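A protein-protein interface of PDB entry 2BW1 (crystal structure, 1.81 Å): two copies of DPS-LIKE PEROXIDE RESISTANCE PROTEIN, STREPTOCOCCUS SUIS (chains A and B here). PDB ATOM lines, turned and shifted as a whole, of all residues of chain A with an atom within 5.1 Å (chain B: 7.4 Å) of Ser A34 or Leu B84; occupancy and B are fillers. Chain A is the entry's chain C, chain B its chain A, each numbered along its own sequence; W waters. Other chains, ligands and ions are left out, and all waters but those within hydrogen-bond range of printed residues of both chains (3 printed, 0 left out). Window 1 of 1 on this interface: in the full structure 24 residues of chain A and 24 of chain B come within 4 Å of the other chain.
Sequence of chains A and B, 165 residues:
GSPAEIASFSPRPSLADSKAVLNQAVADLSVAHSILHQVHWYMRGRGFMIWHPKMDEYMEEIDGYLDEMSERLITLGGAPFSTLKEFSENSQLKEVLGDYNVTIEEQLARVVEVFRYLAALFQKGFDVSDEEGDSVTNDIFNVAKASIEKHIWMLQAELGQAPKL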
ATOM      1  N   LEU A  29       4.572 -15.877 -28.451  1.00  0.00           N
ATOM      2  CA  LEU A  29       4.283 -17.250 -28.870  1.00  0.00           C
ATOM      3  C   LEU A  29       2.902 -17.665 -28.376  1.00  0.00           C
ATOM      4  O   LEU A  29       2.203 -18.420 -29.049  1.00  0.00           O
ATOM      5  CB  LEU A  29       5.364 -18.238 -28.390  1.00  0.00           C
ATOM      6  CG  LEU A  29       6.700 -18.155 -29.140  1.00  0.00           C
ATOM      7  CD1 LEU A  29       7.816 -18.781 -28.295  1.00  0.00           C
ATOM      8  CD2 LEU A  29       6.650 -18.772 -30.545  1.00  0.00           C
ATOM      9  N   SER A  30       2.517 -17.184 -27.194  1.00  0.00           N
ATOM     10  CA  SER A  30       1.158 -17.401 -26.698  1.00  0.00           C
ATOM     11  C   SER A  30       0.084 -16.798 -27.624  1.00  0.00           C
ATOM     12  O   SER A  30      -0.942 -17.419 -27.913  1.00  0.00           O
ATOM     13  CB  SER A  30       1.030 -16.866 -25.279  1.00  0.00           C
ATOM     14  OG  SER A  30       1.911 -17.551 -24.407  1.00  0.00           O
ATOM     15  N   VAL A  31       0.329 -15.573 -28.075  1.00  0.00           N
ATOM     16  CA  VAL A  31      -0.573 -14.908 -29.019  1.00  0.00           C
ATOM     17  C   VAL A  31      -0.526 -15.589 -30.395  1.00  0.00           C
ATOM     18  O   VAL A  31      -1.573 -15.806 -31.014  1.00  0.00           O
ATOM     19  CB  VAL A  31      -0.281 -13.388 -29.114  1.00  0.00           C
ATOM     20  CG1 VAL A  31      -1.162 -12.747 -30.157  1.00  0.00           C
ATOM     21  CG2 VAL A  31      -0.486 -12.736 -27.752  1.00  0.00           C
ATOM     22  N   ALA A  32       0.672 -15.954 -30.868  1.00  0.00           N
ATOM     23  CA  ALA A  32       0.782 -16.684 -32.154  1.00  0.00           C
ATOM     24  C   ALA A  32       0.011 -17.993 -32.143  1.00  0.00           C
ATOM     25  O   ALA A  32      -0.618 -18.336 -33.139  1.00  0.00           O
ATOM     26  CB  ALA A  32       2.256 -16.914 -32.571  1.00  0.00           C
ATOM     27  N   HIS A  33       0.076 -18.728 -31.025  1.00  0.00           N
ATOM     28  CA  HIS A  33      -0.720 -19.961 -30.868  1.00  0.00           C
ATOM     29  C   HIS A  33      -2.192 -19.655 -31.042  1.00  0.00           C
ATOM     30  O   HIS A  33      -2.899 -20.387 -31.742  1.00  0.00           O
ATOM     31  CB  HIS A  33      -0.508 -20.575 -29.486  1.00  0.00           C
ATOM     32  CG  HIS A  33      -1.433 -21.725 -29.177  1.00  0.00           C
ATOM     33  ND1 HIS A  33      -1.054 -23.039 -29.323  1.00  0.00           N
ATOM     34  CD2 HIS A  33      -2.695 -21.750 -28.681  1.00  0.00           C
ATOM     35  CE1 HIS A  33      -2.049 -23.828 -28.948  1.00  0.00           C
ATOM     36  NE2 HIS A  33      -3.056 -23.069 -28.555  1.00  0.00           N
ATOM     37  N   SER A  34      -2.671 -18.595 -30.379  1.00  0.00           N
ATOM     38  CA  SER A  34      -4.074 -18.211 -30.465  1.00  0.00           C
ATOM     39  C   SER A  34      -4.456 -17.836 -31.907  1.00  0.00           C
ATOM     40  O   SER A  34      -5.519 -18.223 -32.412  1.00  0.00           O
ATOM     41  CB  SER A  34      -4.384 -17.061 -29.482  1.00  0.00           C
ATOM     42  OG  SER A  34      -5.766 -16.664 -29.510  1.00  0.00           O
ATOM     43  N   ILE A  35      -3.580 -17.093 -32.576  1.00  0.00           N
ATOM     44  CA  ILE A  35      -3.871 -16.716 -33.953  1.00  0.00           C
ATOM     45  C   ILE A  35      -3.915 -17.942 -34.858  1.00  0.00           C
ATOM     46  O   ILE A  35      -4.863 -18.113 -35.619  1.00  0.00           O
ATOM     47  CB  ILE A  35      -2.889 -15.670 -34.483  1.00  0.00           C
ATOM     48  CG1 ILE A  35      -3.044 -14.340 -33.738  1.00  0.00           C
ATOM     49  CG2 ILE A  35      -3.119 -15.461 -35.982  1.00  0.00           C
ATOM     50  CD1 ILE A  35      -1.906 -13.330 -34.101  1.00  0.00           C
ATOM     51  N   LEU A  36      -2.916 -18.825 -34.747  1.00  0.00           N
ATOM     52  CA  LEU A  36      -2.904 -20.051 -35.557  1.00  0.00           C
ATOM     53  C   LEU A  36      -4.176 -20.864 -35.334  1.00  0.00           C
ATOM     54  O   LEU A  36      -4.699 -21.471 -36.249  1.00  0.00           O
ATOM     55  CB  LEU A  36      -1.665 -20.918 -35.258  1.00  0.00           C
ATOM     56  CG  LEU A  36      -0.284 -20.366 -35.672  1.00  0.00           C
ATOM     57  CD1 LEU A  36       0.874 -21.060 -34.901  1.00  0.00           C
ATOM     58  CD2 LEU A  36      -0.137 -20.566 -37.170  1.00  0.00           C
ATOM     59  N   HIS A  37      -4.652 -20.884 -34.098  1.00  0.00           N
ATOM     60  CA  HIS A  37      -5.856 -21.618 -33.761  1.00  0.00           C
ATOM     61  C   HIS A  37      -7.111 -21.018 -34.392  1.00  0.00           C
ATOM     62  O   HIS A  37      -7.986 -21.728 -34.917  1.00  0.00           O
ATOM     63  CB  HIS A  37      -6.016 -21.706 -32.230  1.00  0.00           C
ATOM     64  CG  HIS A  37      -6.474 -23.050 -31.773  1.00  0.00           C
ATOM     65  ND1 HIS A  37      -6.467 -23.434 -30.450  1.00  0.00           N
ATOM     66  CD2 HIS A  37      -6.907 -24.123 -32.479  1.00  0.00           C
ATOM     67  CE1 HIS A  37      -6.888 -24.687 -30.360  1.00  0.00           C
ATOM     68  NE2 HIS A  37      -7.150 -25.129 -31.577  1.00  0.00           N
ATOM     69  N   GLN A  38      -7.198 -19.700 -34.372  1.00  0.00           N
ATOM     70  CA  GLN A  38      -8.264 -19.017 -35.090  1.00  0.00           C
ATOM     71  C   GLN A  38      -8.275 -19.397 -36.581  1.00  0.00           C
ATOM     72  O   GLN A  38      -9.344 -19.692 -37.128  1.00  0.00           O
ATOM     73  CB  GLN A  38      -8.087 -17.502 -34.989  1.00  0.00           C
ATOM     74  CG  GLN A  38      -9.207 -16.755 -35.692  1.00  0.00           C
ATOM     75  CD  GLN A  38      -9.024 -15.256 -35.573  1.00  0.00           C
ATOM     76  OE1 GLN A  38      -8.401 -14.603 -36.433  1.00  0.00           O
ATOM     77  NE2 GLN A  38      -9.537 -14.712 -34.502  1.00  0.00           N
ATOM     78  N   LEU A  84      -3.109 -14.815 -19.289  1.00  0.00           N
ATOM     79  CA  LEU A  84      -3.500 -14.277 -20.605  1.00  0.00           C
ATOM     80  C   LEU A  84      -3.361 -12.750 -20.663  1.00  0.00           C
ATOM     81  O   LEU A  84      -3.002 -12.205 -21.707  1.00  0.00           O
ATOM     82  CB  LEU A  84      -4.930 -14.666 -20.981  1.00  0.00           C
ATOM     83  CG  LEU A  84      -5.302 -16.154 -21.130  1.00  0.00           C
ATOM     84  CD1 LEU A  84      -6.621 -16.264 -21.868  1.00  0.00           C
ATOM     85  CD2 LEU A  84      -4.190 -17.036 -21.772  1.00  0.00           C
ATOM     86  N   PHE A  87       0.132 -12.032 -21.434  1.00  0.00           N
ATOM     87  CA  PHE A  87       0.494 -12.381 -22.825  1.00  0.00           C
ATOM     88  C   PHE A  87      -0.031 -11.291 -23.765  1.00  0.00           C
ATOM     89  O   PHE A  87       0.689 -10.798 -24.644  1.00  0.00           O
ATOM     90  CB  PHE A  87      -0.087 -13.745 -23.257  1.00  0.00           C
ATOM     91  CG  PHE A  87       0.363 -14.916 -22.414  1.00  0.00           C
ATOM     92  CD1 PHE A  87      -0.504 -16.002 -22.176  1.00  0.00           C
ATOM     93  CD2 PHE A  87       1.643 -14.945 -21.857  1.00  0.00           C
ATOM     94  CE1 PHE A  87      -0.085 -17.099 -21.409  1.00  0.00           C
ATOM     95  CE2 PHE A  87       2.076 -16.030 -21.085  1.00  0.00           C
ATOM     96  CZ  PHE A  87       1.199 -17.115 -20.866  1.00  0.00           C
ATOM     97  N   SER A  88      -1.289 -10.924 -23.548  1.00  0.00           N
ATOM     98  CA  SER A  88      -1.992  -9.984 -24.416  1.00  0.00           C
ATOM     99  C   SER A  88      -1.381  -8.562 -24.337  1.00  0.00           C
ATOM    100  O   SER A  88      -1.174  -7.914 -25.377  1.00  0.00           O
ATOM    101  CB  SER A  88      -3.486 -10.023 -24.089  1.00  0.00           C
ATOM    102  OG  SER A  88      -4.252  -9.589 -25.175  1.00  0.00           O
ATOM    103  N   GLU A  95      -4.612  -9.362 -32.263  1.00  0.00           N
ATOM    104  CA  GLU A  95      -5.637 -10.290 -32.699  1.00  0.00           C
ATOM    105  C   GLU A  95      -6.896  -9.566 -33.127  1.00  0.00           C
ATOM    106  O   GLU A  95      -7.193  -8.462 -32.642  1.00  0.00           O
ATOM    107  CB  GLU A  95      -5.961 -11.261 -31.568  1.00  0.00           C
ATOM    108  CG  GLU A  95      -4.742 -12.099 -31.137  1.00  0.00           C
ATOM    109  CD  GLU A  95      -5.146 -13.059 -30.062  1.00  0.00           C
ATOM    110  OE1 GLU A  95      -5.571 -14.168 -30.428  1.00  0.00           O
ATOM    111  OE2 GLU A  95      -5.050 -12.688 -28.874  1.00  0.00           O
ATOM    112  N   SER B  30      -9.372 -22.419 -22.195  1.00  0.00           N
ATOM    113  CA  SER B  30      -8.254 -21.616 -22.589  1.00  0.00           C
ATOM    114  C   SER B  30      -7.563 -21.016 -21.375  1.00  0.00           C
ATOM    115  O   SER B  30      -6.331 -21.024 -21.308  1.00  0.00           O
ATOM    116  CB  SER B  30      -8.682 -20.523 -23.589  1.00  0.00           C
ATOM    117  OG  SER B  30      -9.088 -21.071 -24.848  1.00  0.00           O
ATOM    118  N   VAL B  31      -8.336 -20.509 -20.408  1.00  0.00           N
ATOM    119  CA  VAL B  31      -7.748 -19.997 -19.156  1.00  0.00           C
ATOM    120  C   VAL B  31      -7.202 -21.158 -18.297  1.00  0.00           C
ATOM    121  O   VAL B  31      -6.109 -21.069 -17.733  1.00  0.00           O
ATOM    122  CB  VAL B  31      -8.759 -19.129 -18.332  1.00  0.00           C
ATOM    123  CG1 VAL B  31      -8.166 -18.684 -16.993  1.00  0.00           C
ATOM    124  CG2 VAL B  31      -9.204 -17.884 -19.156  1.00  0.00           C
ATOM    125  N   PHE B  81     -15.017 -18.305 -29.613  1.00  0.00           N
ATOM    126  CA  PHE B  81     -14.006 -17.369 -29.124  1.00  0.00           C
ATOM    127  C   PHE B  81     -12.652 -17.828 -29.659  1.00  0.00           C
ATOM    128  O   PHE B  81     -12.386 -19.034 -29.725  1.00  0.00           O
ATOM    129  CB  PHE B  81     -13.972 -17.382 -27.595  1.00  0.00           C
ATOM    130  CG  PHE B  81     -15.283 -16.997 -26.946  1.00  0.00           C
ATOM    131  CD1 PHE B  81     -15.763 -17.710 -25.848  1.00  0.00           C
ATOM    132  CD2 PHE B  81     -16.048 -15.948 -27.437  1.00  0.00           C
ATOM    133  CE1 PHE B  81     -16.996 -17.360 -25.232  1.00  0.00           C
ATOM    134  CE2 PHE B  81     -17.263 -15.597 -26.826  1.00  0.00           C
ATOM    135  CZ  PHE B  81     -17.730 -16.293 -25.733  1.00  0.00           C
ATOM    136  N   SER B  82     -11.809 -16.877 -30.071  1.00  0.00           N
ATOM    137  CA  SER B  82     -10.544 -17.225 -30.730  1.00  0.00           C
ATOM    138  C   SER B  82      -9.475 -16.149 -30.594  1.00  0.00           C
ATOM    139  O   SER B  82      -8.576 -16.046 -31.425  1.00  0.00           O
ATOM    140  CB  SER B  82     -10.751 -17.639 -32.191  1.00  0.00           C
ATOM    141  OG  SER B  82     -11.247 -16.561 -32.986  1.00  0.00           O
ATOM    142  N   THR B  83      -9.555 -15.398 -29.496  1.00  0.00           N
ATOM    143  CA  THR B  83      -8.632 -14.323 -29.160  1.00  0.00           C
ATOM    144  C   THR B  83      -8.446 -14.325 -27.659  1.00  0.00           C
ATOM    145  O   THR B  83      -9.368 -14.697 -26.927  1.00  0.00           O
ATOM    146  CB  THR B  83      -9.165 -12.902 -29.579  1.00  0.00           C
ATOM    147  OG1 THR B  83     -10.370 -12.600 -28.859  1.00  0.00           O
ATOM    148  CG2 THR B  83      -9.424 -12.829 -31.096  1.00  0.00           C
ATOM    149  N   LEU B  84      -7.256 -13.959 -27.200  1.00  0.00           N
ATOM    150  CA  LEU B  84      -7.035 -13.881 -25.735  1.00  0.00           C
ATOM    151  C   LEU B  84      -8.018 -12.979 -24.989  1.00  0.00           C
ATOM    152  O   LEU B  84      -8.566 -13.362 -23.934  1.00  0.00           O
ATOM    153  CB  LEU B  84      -5.572 -13.562 -25.395  1.00  0.00           C
ATOM    154  CG  LEU B  84      -4.466 -14.489 -25.918  1.00  0.00           C
ATOM    155  CD1 LEU B  84      -3.141 -14.247 -25.137  1.00  0.00           C
ATOM    156  CD2 LEU B  84      -4.829 -15.991 -25.885  1.00  0.00           C
ATOM    157  N   LYS B  85      -8.292 -11.801 -25.555  1.00  0.00           N
ATOM    158  CA  LYS B  85      -9.371 -10.933 -25.060  1.00  0.00           C
ATOM    159  C   LYS B  85     -10.715 -11.640 -24.827  1.00  0.00           C
ATOM    160  O   LYS B  85     -11.248 -11.537 -23.738  1.00  0.00           O
ATOM    161  CB  LYS B  85      -9.572  -9.719 -25.971  1.00  0.00           C
ATOM    162  CG  LYS B  85     -10.501  -8.685 -25.371  1.00  0.00           C
ATOM    163  CD  LYS B  85     -10.797  -7.565 -26.350  1.00  0.00           C
ATOM    164  CE  LYS B  85     -11.771  -6.586 -25.708  1.00  0.00           C
ATOM    165  NZ  LYS B  85     -13.178  -7.015 -25.937  1.00  0.00           N
ATOM    166  N   GLU B  86     -11.258 -12.347 -25.829  1.00  0.00           N
ATOM    167  CA  GLU B  86     -12.498 -13.132 -25.632  1.00  0.00           C
ATOM    168  C   GLU B  86     -12.390 -14.178 -24.532  1.00  0.00           C
ATOM    169  O   GLU B  86     -13.330 -14.378 -23.743  1.00  0.00           O
ATOM    170  CB  GLU B  86     -12.920 -13.797 -26.937  1.00  0.00           C
ATOM    171  CG  GLU B  86     -13.479 -12.812 -27.949  1.00  0.00           C
ATOM    172  CD  GLU B  86     -13.688 -13.466 -29.259  1.00  0.00           C
ATOM    173  OE1 GLU B  86     -14.855 -13.588 -29.648  1.00  0.00           O
ATOM    174  OE2 GLU B  86     -12.686 -13.917 -29.863  1.00  0.00           O
ATOM    175  N   PHE B  87     -11.242 -14.849 -24.459  1.00  0.00           N
ATOM    176  CA  PHE B  87     -11.092 -15.909 -23.451  1.00  0.00           C
ATOM    177  C   PHE B  87     -11.123 -15.315 -22.038  1.00  0.00           C
ATOM    178  O   PHE B  87     -11.874 -15.794 -21.178  1.00  0.00           O
ATOM    179  CB  PHE B  87      -9.789 -16.722 -23.628  1.00  0.00           C
ATOM    180  CG  PHE B  87      -9.623 -17.407 -24.985  1.00  0.00           C
ATOM    181  CD1 PHE B  87      -8.327 -17.575 -25.515  1.00  0.00           C
ATOM    182  CD2 PHE B  87     -10.720 -17.887 -25.721  1.00  0.00           C
ATOM    183  CE1 PHE B  87      -8.129 -18.226 -26.769  1.00  0.00           C
ATOM    184  CE2 PHE B  87     -10.520 -18.538 -26.977  1.00  0.00           C
ATOM    185  CZ  PHE B  87      -9.219 -18.699 -27.491  1.00  0.00           C
ATOM    186  N   SER B  88     -10.304 -14.288 -21.800  1.00  0.00           N
ATOM    187  CA  SER B  88     -10.197 -13.622 -20.478  1.00  0.00           C
ATOM    188  C   SER B  88     -11.526 -13.047 -19.998  1.00  0.00           C
ATOM    189  O   SER B  88     -11.940 -13.268 -18.849  1.00  0.00           O
ATOM    190  CB  SER B  88      -9.209 -12.452 -20.551  1.00  0.00           C
ATOM    191  OG  SER B  88      -7.879 -12.896 -20.565  1.00  0.00           O
ATOM    192  N   GLU B  89     -12.206 -12.363 -20.902  1.00  0.00           N
ATOM    193  CA  GLU B  89     -13.424 -11.615 -20.598  1.00  0.00           C
ATOM    194  C   GLU B  89     -14.656 -12.492 -20.481  1.00  0.00           C
ATOM    195  O   GLU B  89     -15.641 -12.106 -19.841  1.00  0.00           O
ATOM    196  CB  GLU B  89     -13.644 -10.536 -21.651  1.00  0.00           C
ATOM    197  CG  GLU B  89     -12.577  -9.452 -21.593  1.00  0.00           C
ATOM    198  CD  GLU B  89     -12.811  -8.349 -22.601  1.00  0.00           C
ATOM    199  OE1 GLU B  89     -12.163  -7.281 -22.478  1.00  0.00           O
ATOM    200  OE2 GLU B  89     -13.630  -8.548 -23.516  1.00  0.00           O
ATOM    201  N   ASN B  90     -14.632 -13.653 -21.120  1.00  0.00           N
ATOM    202  CA  ASN B  90     -15.739 -14.606 -20.967  1.00  0.00           C
ATOM    203  C   ASN B  90     -15.515 -15.680 -19.928  1.00  0.00           C
ATOM    204  O   ASN B  90     -16.498 -16.251 -19.433  1.00  0.00           O
ATOM    205  CB  ASN B  90     -16.093 -15.257 -22.297  1.00  0.00           C
ATOM    206  CG  ASN B  90     -16.749 -14.296 -23.235  1.00  0.00           C
ATOM    207  OD1 ASN B  90     -17.959 -14.103 -23.173  1.00  0.00           O
ATOM    208  ND2 ASN B  90     -15.964 -13.675 -24.104  1.00  0.00           N
HETATM  209  O   HOH W   1      -7.074 -10.683 -27.831  1.00  0.00           O
HETATM  210  O   HOH W   2      -7.424 -18.756 -30.452  1.00  0.00           O
HETATM  211  O   HOH W   3      -6.466 -14.677 -32.875  1.00  0.00           O
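Of the 14 printed residues of chain A, 5 touch a printed residue of chain B.
Among the printed residues, no Asp or Glu carboxylate lies within 4 Å of a Lys or Arg side-chain nitrogen of the other chain.
Thr B83 touches Ser A34.
Ser A34 touches Leu B84.
CE1 of Phe B87 touches OG of Ser A34, at 3.9 Å.
Thr B83 touches Gln A38 (CG2 to NE2, 3.9 Å).
Leu A84 touches Leu B84.
CB of Phe B87 touches CD1 of Leu A84 (3.7 Å).
CB of Leu A84 touches OG of Ser B88 (3.5 Å).
Leu B84 touches Phe A87.
Glu A95 touches Ser B82 (OE1 to O, 3.7 Å).
OE1 of Glu A95 touches CA of Thr B83, at 3.3 Å.
Leu B84 touches its own counterpart, Leu A84.
Leu A84 touches Phe B87, and with the chains exchanged Phe A87 touches Leu B84.
Leu A84 touches Ser B88, but with the chains exchanged Ser A88 does not touch Leu B84 (4.1 Å).
Positions printed for both chains: 30, 31, 84, 87 and 88.
Of the 13 pairs that touch across the chains among the printed residues, 3 have their exchanged pair printed and touching as well.
Of chain B, only Ser B82, Thr B83, Leu B84 and Phe B87 come within 4 Å of Ser A34.
His A37 touches none of the printed residues of chain B.
Printed residues of chain B within 4 Å of Leu A84: Leu B84 (3.99 Å), Phe B87 (3.7 Å) and Ser B88 (3.5 Å).
Of the printed residues of chain B, Phe A87 touches Leu B84 (3.6 Å).
Ser B30 touches none of the printed residues of chain A.
Of the printed residues of chain A, Leu B84 touches Ser A34 (3.8 Å), Leu A84 (3.99 Å), Phe A87 (3.6 Å) and Glu A95 (3.0 Å).
The nearest residue of chain B that does not touch Ser A34 is Lys B85 (6.8 Å).
The nearest printed residue of chain B that does not touch Leu A84 is Val B31 (4.1 Å).
Water W3 lies within hydrogen-bond range of the side-chain carboxylate (OE1) of Glu A95 (2.7 Å), the backbone carbonyl oxygen (O) of Ser B82 (2.9 Å) and the side-chain amide nitrogen (NE2) of Gln A38 (3.5 Å).
Water W2 lies within hydrogen-bond range of O of Ser A34 and O of Ser B82.
Water W1 lies within hydrogen-bond range of N of Lys B85 (2.8 Å), OE2 of Glu A95 (3.0 Å) and N of Leu B84 (3.3 Å).
The side-chain hydroxyl (OG) of Ser A34 is in hydrogen-bond range of the side-chain carboxylate (OE1) of Glu A95, 2.7 Å away.
N of Ser B82 sits at hydrogen-bond distance from OE2 of Glu B86 (3.1 Å).
OE2 of Glu B86 lies within hydrogen-bond range of OG1 of Thr B83 (2.8 Å).
The side-chain hydroxyl of Ser B88 sits at hydrogen-bond distance from the backbone carbonyl oxygen of Leu B84, 3.5 Å away.
O of Ser B82 lies within hydrogen-bond range of OG of Ser A34.
N of Leu B84 is in hydrogen-bond range of OE2 of Glu A95 (3.0 Å).
NE2 of Gln A38 sits at hydrogen-bond distance from OG of Ser B82 (2.9 Å).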
